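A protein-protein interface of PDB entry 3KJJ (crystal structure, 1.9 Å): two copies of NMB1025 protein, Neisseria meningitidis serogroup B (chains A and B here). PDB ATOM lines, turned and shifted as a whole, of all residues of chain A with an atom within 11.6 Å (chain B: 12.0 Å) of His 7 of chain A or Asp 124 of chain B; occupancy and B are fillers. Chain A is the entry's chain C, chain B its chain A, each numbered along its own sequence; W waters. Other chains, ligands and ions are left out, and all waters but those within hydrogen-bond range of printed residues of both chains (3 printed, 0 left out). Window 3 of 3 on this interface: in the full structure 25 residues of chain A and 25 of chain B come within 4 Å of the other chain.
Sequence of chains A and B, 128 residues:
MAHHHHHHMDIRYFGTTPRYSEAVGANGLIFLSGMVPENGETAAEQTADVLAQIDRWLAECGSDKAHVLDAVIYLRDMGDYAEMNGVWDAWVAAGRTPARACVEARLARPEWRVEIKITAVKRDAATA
The side-chain carboxylate of Asp 124 of chain B sits at hydrogen-bond distance from the backbone NH of His 7 of chain A (3.3 Å). The side-chain carboxylate (OD2) of Asp 124 of chain B sits at hydrogen-bond distance from the backbone NH (N) of His 8 of chain A, 3.2 Å away. The side-chain carboxylate of Asp 124 of chain B sits at hydrogen-bond distance from the backbone NH of Met 9 of chain A.
The backbone carbonyl oxygen (O) of His 8 of chain B sits close to the side-chain amide oxygen (OD1) of Asn 27 of chain B, 2.8 Å away. The backbone carbonyl oxygen of Gly 28 of chain B sits at hydrogen-bond distance from the backbone NH of Lys 122 of chain B (2.8 Å). O of Val 121 of chain B lies within hydrogen-bond range of OG of Ser 63 of chain B (2.7 Å). OD1 of Asp 64 of chain B sits at hydrogen-bond distance from ND1 of His 67 of chain B (2.8 Å). The guanidinium group (NE) of Arg 96 of chain B is in hydrogen-bond range of the backbone carbonyl oxygen (O) of Ala 66 of chain B. O of His 67 of chain B lies within hydrogen-bond range of N of Val 121 of chain B, 3.0 Å away.
Among the printed residues, pairs that only touch across the chains: Met 9 of chain A with Asn 27 of chain B, Met 9 of chain A with Val 121 of chain B, Met 9 of chain A with Lys 122 of chain B, Ile 11 of chain A with His 67 of chain B, Ile 11 of chain A with Arg 96 of chain B, Ile 11 of chain A with Val 121 of chain B, Ala 26 of chain A with Leu 69 of chain B and Leu 29 of chain A with Leu 29 of chain B.
Of chain B, only Asp 124 (3.3 Å) comes within 4 Å of His 7 of chain A. Of chain A, only His 7 (3.3 Å), His 8 (3.2 Å) and Met 9 (3.0 Å) come within 4 Å of Asp 124 of chain B. His 8 of chain A touches just one residue of chain B: Asp 124. No residue of chain B comes within 4 Å of Asp 10 of chain A. No residue of chain A comes within 4 Å of Gly 28 of chain B. Lys 122 of chain B touches just one residue of chain A: Met 9. Printed residues of chain B within 4 Å of Leu 29 of chain A: Leu 29 (3.6 Å). Printed residues of chain A within 4 Å of Arg 96 of chain B: Ile 11 (3.7 Å). Ala 26 of chain B touches none of the printed residues of chain A. Ser 63 of chain B touches none of the printed residues of chain A.
Of the 12 printed residues of chain A, 6 touch a printed residue of chain B. Of the 22 printed residues of chain B, 8 touch a printed residue of chain A. Among the printed residues, 11 pairs touch across the chains. Among the printed residues, no Asp or Glu carboxylate lies within 4 Å of a Lys or Arg side-chain nitrogen of the other chain.
Leu 29 of chain A touches its own counterpart, Leu 29 of chain B. Positions printed for both chains: 8, 26, 27, 28, 29 and 122.
Water W2 lies within hydrogen-bond range of the guanidinium group (NH2) of Arg 96 of chain B (2.6 Å) and the backbone NH (N) of Ile 11 of chain A (3.3 Å). Water W1 bridges OD1 of Asp 10 of chain A and OD2 of Asp 124 of chain B. Water W3 lies within hydrogen-bond range of ND2 of Asn 27 of chain A (3.0 Å), O of Asn 27 of chain B (3.3 Å) and SD of Met 9 of chain A (3.4 Å).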
ATOM      1  N   HIS A   7      20.689 -26.579 -30.149  1.00  0.00           N
ATOM      2  CA  HIS A   7      21.389 -27.897 -30.129  1.00  0.00           C
ATOM      3  C   HIS A   7      22.908 -27.736 -30.043  1.00  0.00           C
ATOM      4  O   HIS A   7      23.652 -28.723 -30.094  1.00  0.00           O
ATOM      5  CB  HIS A   7      20.999 -28.736 -31.349  1.00  0.00           C
ATOM      6  N   HIS A   8      23.354 -26.487 -29.900  1.00  0.00           N
ATOM      7  CA  HIS A   8      24.775 -26.160 -29.754  1.00  0.00           C
ATOM      8  C   HIS A   8      25.412 -26.915 -28.580  1.00  0.00           C
ATOM      9  O   HIS A   8      26.552 -27.376 -28.673  1.00  0.00           O
ATOM     10  CB  HIS A   8      24.941 -24.644 -29.586  1.00  0.00           C
ATOM     11  CG  HIS A   8      26.306 -24.131 -29.934  1.00  0.00           C
ATOM     12  ND1 HIS A   8      27.117 -24.731 -30.878  1.00  0.00           N
ATOM     13  CD2 HIS A   8      26.987 -23.045 -29.489  1.00  0.00           C
ATOM     14  CE1 HIS A   8      28.248 -24.051 -30.980  1.00  0.00           C
ATOM     15  NE2 HIS A   8      28.194 -23.025 -30.147  1.00  0.00           N
ATOM     16  N   MET A   9      24.652 -27.066 -27.500  1.00  0.00           N
ATOM     17  CA  MET A   9      25.131 -27.726 -26.286  1.00  0.00           C
ATOM     18  C   MET A   9      24.596 -29.158 -26.089  1.00  0.00           C
ATOM     19  O   MET A   9      24.477 -29.621 -24.949  1.00  0.00           O
ATOM     20  CB  MET A   9      24.798 -26.868 -25.053  1.00  0.00           C
ATOM     21  CG  MET A   9      25.114 -25.382 -25.191  1.00  0.00           C
ATOM     22  SD  MET A   9      26.976 -25.042 -25.668  1.00  0.00           S
ATOM     23  CE  MET A   9      26.756 -23.275 -26.431  1.00  0.00           C
ATOM     24  N   ASP A  10      24.289 -29.858 -27.189  1.00  0.00           N
ATOM     25  CA  ASP A  10      23.851 -31.261 -27.122  1.00  0.00           C
ATOM     26  C   ASP A  10      24.875 -32.107 -26.375  1.00  0.00           C
ATOM     27  O   ASP A  10      26.081 -31.970 -26.587  1.00  0.00           O
ATOM     28  CB  ASP A  10      23.662 -31.865 -28.519  1.00  0.00           C
ATOM     29  CG  ASP A  10      22.415 -31.360 -29.234  1.00  0.00           C
ATOM     30  OD1 ASP A  10      21.490 -30.835 -28.579  1.00  0.00           O
ATOM     31  OD2 ASP A  10      22.364 -31.504 -30.474  1.00  0.00           O
ATOM     32  N   ILE A  11      24.390 -32.984 -25.506  1.00  0.00           N
ATOM     33  CA  ILE A  11      25.269 -33.888 -24.784  1.00  0.00           C
ATOM     34  C   ILE A  11      25.254 -35.294 -25.383  1.00  0.00           C
ATOM     35  O   ILE A  11      24.193 -35.876 -25.642  1.00  0.00           O
ATOM     36  CB  ILE A  11      24.942 -33.939 -23.277  1.00  0.00           C
ATOM     37  CG1 ILE A  11      24.889 -32.521 -22.690  1.00  0.00           C
ATOM     38  CG2 ILE A  11      26.002 -34.741 -22.539  1.00  0.00           C
ATOM     39  CD1 ILE A  11      24.267 -32.450 -21.292  1.00  0.00           C
ATOM     40  N   ARG A  12      26.451 -35.825 -25.607  1.00  0.00           N
ATOM     41  CA  ARG A  12      26.622 -37.199 -26.024  1.00  0.00           C
ATOM     42  C   ARG A  12      27.189 -37.972 -24.827  1.00  0.00           C
ATOM     43  O   ARG A  12      28.082 -37.483 -24.133  1.00  0.00           O
ATOM     44  CB  ARG A  12      27.552 -37.272 -27.244  1.00  0.00           C
ATOM     45  CG  ARG A  12      27.670 -38.676 -27.852  1.00  0.00           C
ATOM     46  CD  ARG A  12      27.128 -38.782 -29.271  1.00  0.00           C
ATOM     47  NE  ARG A  12      27.434 -40.100 -29.837  1.00  0.00           N
ATOM     48  CZ  ARG A  12      28.540 -40.397 -30.518  1.00  0.00           C
ATOM     49  NH1 ARG A  12      29.462 -39.469 -30.747  1.00  0.00           N
ATOM     50  NH2 ARG A  12      28.723 -41.629 -30.978  1.00  0.00           N
ATOM     51  N   GLY A  25      30.423 -35.821 -23.718  1.00  0.00           N
ATOM     52  CA  GLY A  25      30.847 -34.757 -24.623  1.00  0.00           C
ATOM     53  C   GLY A  25      29.784 -33.700 -24.873  1.00  0.00           C
ATOM     54  O   GLY A  25      28.610 -34.031 -25.072  1.00  0.00           O
ATOM     55  N   ALA A  26      30.206 -32.436 -24.851  1.00  0.00           N
ATOM     56  CA  ALA A  26      29.360 -31.295 -25.220  1.00  0.00           C
ATOM     57  C   ALA A  26      30.185 -30.147 -25.795  1.00  0.00           C
ATOM     58  O   ALA A  26      31.225 -29.786 -25.246  1.00  0.00           O
ATOM     59  CB  ALA A  26      28.547 -30.805 -24.033  1.00  0.00           C
ATOM     60  N   ASN A  27      29.700 -29.587 -26.905  1.00  0.00           N
ATOM     61  CA  ASN A  27      30.324 -28.452 -27.588  1.00  0.00           C
ATOM     62  C   ASN A  27      31.849 -28.551 -27.721  1.00  0.00           C
ATOM     63  O   ASN A  27      32.564 -27.577 -27.509  1.00  0.00           O
ATOM     64  CB  ASN A  27      29.912 -27.128 -26.933  1.00  0.00           C
ATOM     65  CG  ASN A  27      30.118 -25.924 -27.849  1.00  0.00           C
ATOM     66  OD1 ASN A  27      29.966 -26.018 -29.071  1.00  0.00           O
ATOM     67  ND2 ASN A  27      30.459 -24.784 -27.256  1.00  0.00           N
ATOM     68  N   GLY A  28      32.333 -29.740 -28.063  1.00  0.00           N
ATOM     69  CA  GLY A  28      33.750 -29.938 -28.330  1.00  0.00           C
ATOM     70  C   GLY A  28      34.537 -30.472 -27.153  1.00  0.00           C
ATOM     71  O   GLY A  28      35.568 -31.098 -27.352  1.00  0.00           O
ATOM     72  N   LEU A  29      34.038 -30.239 -25.938  1.00  0.00           N
ATOM     73  CA  LEU A  29      34.717 -30.667 -24.715  1.00  0.00           C
ATOM     74  C   LEU A  29      34.352 -32.093 -24.359  1.00  0.00           C
ATOM     75  O   LEU A  29      33.256 -32.557 -24.656  1.00  0.00           O
ATOM     76  CB  LEU A  29      34.368 -29.756 -23.539  1.00  0.00           C
ATOM     77  CG  LEU A  29      34.826 -28.301 -23.591  1.00  0.00           C
ATOM     78  CD1 LEU A  29      33.921 -27.473 -22.727  1.00  0.00           C
ATOM     79  CD2 LEU A  29      36.284 -28.168 -23.163  1.00  0.00           C
ATOM     80  N   LYS A 122      37.515 -32.542 -28.451  1.00  0.00           N
ATOM     81  CA  LYS A 122      37.269 -33.295 -29.662  1.00  0.00           C
ATOM     82  C   LYS A 122      37.967 -32.580 -30.806  1.00  0.00           C
ATOM     83  O   LYS A 122      37.667 -31.416 -31.103  1.00  0.00           O
ATOM     84  CB  LYS A 122      35.757 -33.409 -29.916  1.00  0.00           C
ATOM     85  CG  LYS A 122      35.354 -34.208 -31.159  1.00  0.00           C
ATOM     86  CD  LYS A 122      33.831 -34.399 -31.224  1.00  0.00           C
ATOM     87  CE  LYS A 122      33.422 -35.198 -32.455  1.00  0.00           C
ATOM     88  NZ  LYS A 122      31.964 -35.526 -32.487  1.00  0.00           N
ATOM     89  N   HIS B   8      30.557 -13.347 -26.348  1.00  0.00           N
ATOM     90  CA  HIS B   8      30.580 -14.830 -26.488  1.00  0.00           C
ATOM     91  C   HIS B   8      31.054 -15.505 -25.199  1.00  0.00           C
ATOM     92  O   HIS B   8      30.470 -16.494 -24.749  1.00  0.00           O
ATOM     93  CB  HIS B   8      31.461 -15.248 -27.666  1.00  0.00           C
ATOM     94  N   ALA B  26      29.327 -19.499 -18.438  1.00  0.00           N
ATOM     95  CA  ALA B  26      30.014 -18.894 -19.579  1.00  0.00           C
ATOM     96  C   ALA B  26      29.887 -19.796 -20.802  1.00  0.00           C
ATOM     97  O   ALA B  26      30.201 -20.991 -20.737  1.00  0.00           O
ATOM     98  CB  ALA B  26      31.488 -18.631 -19.266  1.00  0.00           C
ATOM     99  N   ASN B  27      29.423 -19.207 -21.907  1.00  0.00           N
ATOM    100  CA  ASN B  27      29.262 -19.896 -23.195  1.00  0.00           C
ATOM    101  C   ASN B  27      28.634 -21.297 -23.108  1.00  0.00           C
ATOM    102  O   ASN B  27      29.198 -22.289 -23.603  1.00  0.00           O
ATOM    103  CB  ASN B  27      30.586 -19.925 -23.969  1.00  0.00           C
ATOM    104  CG  ASN B  27      30.381 -19.869 -25.483  1.00  0.00           C
ATOM    105  OD1 ASN B  27      29.885 -18.875 -26.022  1.00  0.00           O
ATOM    106  ND2 ASN B  27      30.771 -20.928 -26.170  1.00  0.00           N
ATOM    107  N   GLY B  28      27.469 -21.365 -22.470  1.00  0.00           N
ATOM    108  CA  GLY B  28      26.699 -22.612 -22.372  1.00  0.00           C
ATOM    109  C   GLY B  28      27.100 -23.527 -21.227  1.00  0.00           C
ATOM    110  O   GLY B  28      26.377 -24.467 -20.901  1.00  0.00           O
ATOM    111  N   LEU B  29      28.249 -23.262 -20.616  1.00  0.00           N
ATOM    112  CA  LEU B  29      28.720 -24.081 -19.501  1.00  0.00           C
ATOM    113  C   LEU B  29      28.314 -23.497 -18.168  1.00  0.00           C
ATOM    114  O   LEU B  29      28.209 -22.285 -18.021  1.00  0.00           O
ATOM    115  CB  LEU B  29      30.236 -24.254 -19.544  1.00  0.00           C
ATOM    116  CG  LEU B  29      30.848 -25.230 -20.539  1.00  0.00           C
ATOM    117  CD1 LEU B  29      32.364 -25.055 -20.536  1.00  0.00           C
ATOM    118  CD2 LEU B  29      30.466 -26.666 -20.205  1.00  0.00           C
ATOM    119  N   ILE B  30      28.082 -24.377 -17.197  1.00  0.00           N
ATOM    120  CA  ILE B  30      27.777 -23.972 -15.841  1.00  0.00           C
ATOM    121  C   ILE B  30      28.742 -24.657 -14.871  1.00  0.00           C
ATOM    122  O   ILE B  30      28.924 -25.872 -14.925  1.00  0.00           O
ATOM    123  CB  ILE B  30      26.305 -24.312 -15.467  1.00  0.00           C
ATOM    124  CG1 ILE B  30      25.342 -23.492 -16.341  1.00  0.00           C
ATOM    125  CG2 ILE B  30      26.056 -24.022 -13.999  1.00  0.00           C
ATOM    126  CD1 ILE B  30      23.941 -24.072 -16.471  1.00  0.00           C
ATOM    127  N   LEU B  58      20.977 -25.539 -10.447  1.00  0.00           N
ATOM    128  CA  LEU B  58      20.852 -25.919 -11.851  1.00  0.00           C
ATOM    129  C   LEU B  58      19.636 -25.220 -12.482  1.00  0.00           C
ATOM    130  O   LEU B  58      19.772 -24.536 -13.504  1.00  0.00           O
ATOM    131  CB  LEU B  58      20.810 -27.452 -12.034  1.00  0.00           C
ATOM    132  CG  LEU B  58      22.120 -28.236 -11.805  1.00  0.00           C
ATOM    133  CD1 LEU B  58      21.980 -29.709 -12.193  1.00  0.00           C
ATOM    134  CD2 LEU B  58      23.308 -27.619 -12.552  1.00  0.00           C
ATOM    135  N   ALA B  59      18.478 -25.349 -11.838  1.00  0.00           N
ATOM    136  CA  ALA B  59      17.231 -24.770 -12.334  1.00  0.00           C
ATOM    137  C   ALA B  59      17.363 -23.263 -12.526  1.00  0.00           C
ATOM    138  O   ALA B  59      17.015 -22.737 -13.577  1.00  0.00           O
ATOM    139  CB  ALA B  59      16.079 -25.092 -11.396  1.00  0.00           C
ATOM    140  N   CYS B  61      19.948 -21.698 -13.197  1.00  0.00           N
ATOM    141  CA  CYS B  61      20.875 -21.441 -14.302  1.00  0.00           C
ATOM    142  C   CYS B  61      20.397 -21.932 -15.668  1.00  0.00           C
ATOM    143  O   CYS B  61      21.162 -21.885 -16.626  1.00  0.00           O
ATOM    144  CB  CYS B  61      22.241 -22.074 -14.010  1.00  0.00           C
ATOM    145  SG  CYS B  61      23.014 -21.469 -12.512  1.00  0.00           S
ATOM    146  N   GLY B  62      19.160 -22.422 -15.757  1.00  0.00           N
ATOM    147  CA  GLY B  62      18.612 -22.930 -17.022  1.00  0.00           C
ATOM    148  C   GLY B  62      19.085 -24.335 -17.376  1.00  0.00           C
ATOM    149  O   GLY B  62      19.167 -24.702 -18.545  1.00  0.00           O
ATOM    150  N   SER B  63      19.395 -25.122 -16.350  1.00  0.00           N
ATOM    151  CA  SER B  63      19.886 -26.478 -16.519  1.00  0.00           C
ATOM    152  C   SER B  63      19.078 -27.421 -15.633  1.00  0.00           C
ATOM    153  O   SER B  63      18.090 -27.011 -15.022  1.00  0.00           O
ATOM    154  CB  SER B  63      21.370 -26.531 -16.140  1.00  0.00           C
ATOM    155  OG  SER B  63      21.944 -27.775 -16.469  1.00  0.00           O
ATOM    156  N   ASP B  64      19.488 -28.689 -15.604  1.00  0.00           N
ATOM    157  CA  ASP B  64      18.963 -29.692 -14.674  1.00  0.00           C
ATOM    158  C   ASP B  64      19.925 -30.884 -14.588  1.00  0.00           C
ATOM    159  O   ASP B  64      20.971 -30.906 -15.254  1.00  0.00           O
ATOM    160  CB  ASP B  64      17.542 -30.149 -15.072  1.00  0.00           C
ATOM    161  CG  ASP B  64      17.465 -30.644 -16.505  1.00  0.00           C
ATOM    162  OD1 ASP B  64      18.281 -31.507 -16.889  1.00  0.00           O
ATOM    163  OD2 ASP B  64      16.582 -30.173 -17.255  1.00  0.00           O
ATOM    164  N   ALA B  66      19.736 -33.891 -15.685  1.00  0.00           N
ATOM    165  CA  ALA B  66      19.909 -34.586 -16.963  1.00  0.00           C
ATOM    166  C   ALA B  66      20.839 -33.839 -17.936  1.00  0.00           C
ATOM    167  O   ALA B  66      21.047 -34.282 -19.064  1.00  0.00           O
ATOM    168  CB  ALA B  66      18.549 -34.867 -17.609  1.00  0.00           C
ATOM    169  N   HIS B  67      21.389 -32.708 -17.496  1.00  0.00           N
ATOM    170  CA  HIS B  67      22.397 -31.986 -18.279  1.00  0.00           C
ATOM    171  C   HIS B  67      23.660 -31.696 -17.470  1.00  0.00           C
ATOM    172  O   HIS B  67      24.368 -30.714 -17.725  1.00  0.00           O
ATOM    173  CB  HIS B  67      21.811 -30.704 -18.870  1.00  0.00           C
ATOM    174  CG  HIS B  67      20.709 -30.953 -19.846  1.00  0.00           C
ATOM    175  ND1 HIS B  67      19.452 -31.357 -19.454  1.00  0.00           N
ATOM    176  CD2 HIS B  67      20.675 -30.870 -21.197  1.00  0.00           C
ATOM    177  CE1 HIS B  67      18.689 -31.512 -20.522  1.00  0.00           C
ATOM    178  NE2 HIS B  67      19.409 -31.230 -21.591  1.00  0.00           N
ATOM    179  N   VAL B  68      23.928 -32.559 -16.490  1.00  0.00           N
ATOM    180  CA  VAL B  68      25.217 -32.563 -15.799  1.00  0.00           C
ATOM    181  C   VAL B  68      26.239 -33.309 -16.646  1.00  0.00           C
ATOM    182  O   VAL B  68      25.990 -34.428 -17.119  1.00  0.00           O
ATOM    183  CB  VAL B  68      25.122 -33.206 -14.398  1.00  0.00           C
ATOM    184  CG1 VAL B  68      26.491 -33.289 -13.738  1.00  0.00           C
ATOM    185  CG2 VAL B  68      24.170 -32.419 -13.515  1.00  0.00           C
ATOM    186  N   LEU B  69      27.393 -32.671 -16.824  1.00  0.00           N
ATOM    187  CA  LEU B  69      28.501 -33.219 -17.587  1.00  0.00           C
ATOM    188  C   LEU B  69      29.378 -34.045 -16.667  1.00  0.00           C
ATOM    189  O   LEU B  69      29.767 -35.172 -16.993  1.00  0.00           O
ATOM    190  CB  LEU B  69      29.361 -32.078 -18.143  1.00  0.00           C
ATOM    191  CG  LEU B  69      28.754 -31.182 -19.227  1.00  0.00           C
ATOM    192  CD1 LEU B  69      29.609 -29.970 -19.457  1.00  0.00           C
ATOM    193  CD2 LEU B  69      28.555 -31.946 -20.521  1.00  0.00           C
ATOM    194  N   ARG B  96      21.315 -40.700 -18.779  1.00  0.00           N
ATOM    195  CA  ARG B  96      22.011 -39.418 -18.964  1.00  0.00           C
ATOM    196  C   ARG B  96      22.841 -39.088 -17.724  1.00  0.00           C
ATOM    197  O   ARG B  96      22.782 -37.975 -17.197  1.00  0.00           O
ATOM    198  CB  ARG B  96      21.005 -38.295 -19.241  1.00  0.00           C
ATOM    199  CG  ARG B  96      20.318 -38.403 -20.601  1.00  0.00           C
ATOM    200  CD  ARG B  96      19.424 -37.214 -20.866  1.00  0.00           C
ATOM    201  NE  ARG B  96      20.182 -35.975 -21.006  1.00  0.00           N
ATOM    202  CZ  ARG B  96      20.458 -35.382 -22.165  1.00  0.00           C
ATOM    203  NH1 ARG B  96      20.041 -35.912 -23.312  1.00  0.00           N
ATOM    204  NH2 ARG B  96      21.152 -34.250 -22.175  1.00  0.00           N
ATOM    205  N   ALA B 120      27.960 -28.374 -15.462  1.00  0.00           N
ATOM    206  CA  ALA B 120      26.761 -28.657 -16.253  1.00  0.00           C
ATOM    207  C   ALA B 120      26.663 -27.818 -17.526  1.00  0.00           C
ATOM    208  O   ALA B 120      27.466 -26.913 -17.756  1.00  0.00           O
ATOM    209  CB  ALA B 120      25.517 -28.485 -15.405  1.00  0.00           C
ATOM    210  N   VAL B 121      25.677 -28.140 -18.356  1.00  0.00           N
ATOM    211  CA  VAL B 121      25.373 -27.327 -19.522  1.00  0.00           C
ATOM    212  C   VAL B 121      24.003 -26.654 -19.407  1.00  0.00           C
ATOM    213  O   VAL B 121      23.033 -27.258 -18.930  1.00  0.00           O
ATOM    214  CB  VAL B 121      25.493 -28.142 -20.822  1.00  0.00           C
ATOM    215  CG1 VAL B 121      24.174 -28.816 -21.187  1.00  0.00           C
ATOM    216  CG2 VAL B 121      26.013 -27.265 -21.954  1.00  0.00           C
ATOM    217  N   LYS B 122      23.949 -25.399 -19.843  1.00  0.00           N
ATOM    218  CA  LYS B 122      22.707 -24.656 -19.968  1.00  0.00           C
ATOM    219  C   LYS B 122      21.936 -25.194 -21.171  1.00  0.00           C
ATOM    220  O   LYS B 122      22.460 -25.212 -22.292  1.00  0.00           O
ATOM    221  CB  LYS B 122      23.001 -23.161 -20.150  1.00  0.00           C
ATOM    222  CG  LYS B 122      21.753 -22.269 -20.195  1.00  0.00           C
ATOM    223  CD  LYS B 122      22.093 -20.883 -20.726  1.00  0.00           C
ATOM    224  CE  LYS B 122      20.918 -19.918 -20.600  1.00  0.00           C
ATOM    225  NZ  LYS B 122      19.872 -20.153 -21.632  1.00  0.00           N
ATOM    226  N   ARG B 123      20.708 -25.649 -20.921  1.00  0.00           N
ATOM    227  CA  ARG B 123      19.791 -26.089 -21.975  1.00  0.00           C
ATOM    228  C   ARG B 123      19.594 -25.006 -23.025  1.00  0.00           C
ATOM    229  O   ARG B 123      19.481 -23.822 -22.702  1.00  0.00           O
ATOM    230  CB  ARG B 123      18.431 -26.476 -21.381  1.00  0.00           C
ATOM    231  CG  ARG B 123      18.387 -27.862 -20.780  1.00  0.00           C
ATOM    232  CD  ARG B 123      17.505 -27.921 -19.546  1.00  0.00           C
ATOM    233  NE  ARG B 123      16.121 -27.524 -19.807  1.00  0.00           N
ATOM    234  CZ  ARG B 123      15.229 -27.231 -18.862  1.00  0.00           C
ATOM    235  NH1 ARG B 123      15.561 -27.280 -17.575  1.00  0.00           N
ATOM    236  NH2 ARG B 123      13.997 -26.880 -19.208  1.00  0.00           N
ATOM    237  N   ASP B 124      19.566 -25.420 -24.287  1.00  0.00           N
ATOM    238  CA  ASP B 124      19.298 -24.503 -25.390  1.00  0.00           C
ATOM    239  C   ASP B 124      17.814 -24.169 -25.456  1.00  0.00           C
ATOM    240  O   ASP B 124      16.964 -24.986 -25.093  1.00  0.00           O
ATOM    241  CB  ASP B 124      19.777 -25.102 -26.713  1.00  0.00           C
ATOM    242  CG  ASP B 124      21.290 -25.147 -26.818  1.00  0.00           C
ATOM    243  OD1 ASP B 124      21.927 -24.083 -26.681  1.00  0.00           O
ATOM    244  OD2 ASP B 124      21.847 -26.246 -27.041  1.00  0.00           O
HETATM  245  O   HOH W   1      20.890 -28.739 -27.038  1.00  0.00           O
HETATM  246  O   HOH W   2      21.286 -32.823 -24.316  1.00  0.00           O
HETATM  247  O   HOH W   3      30.058 -25.338 -24.334  1.00  0.00           O
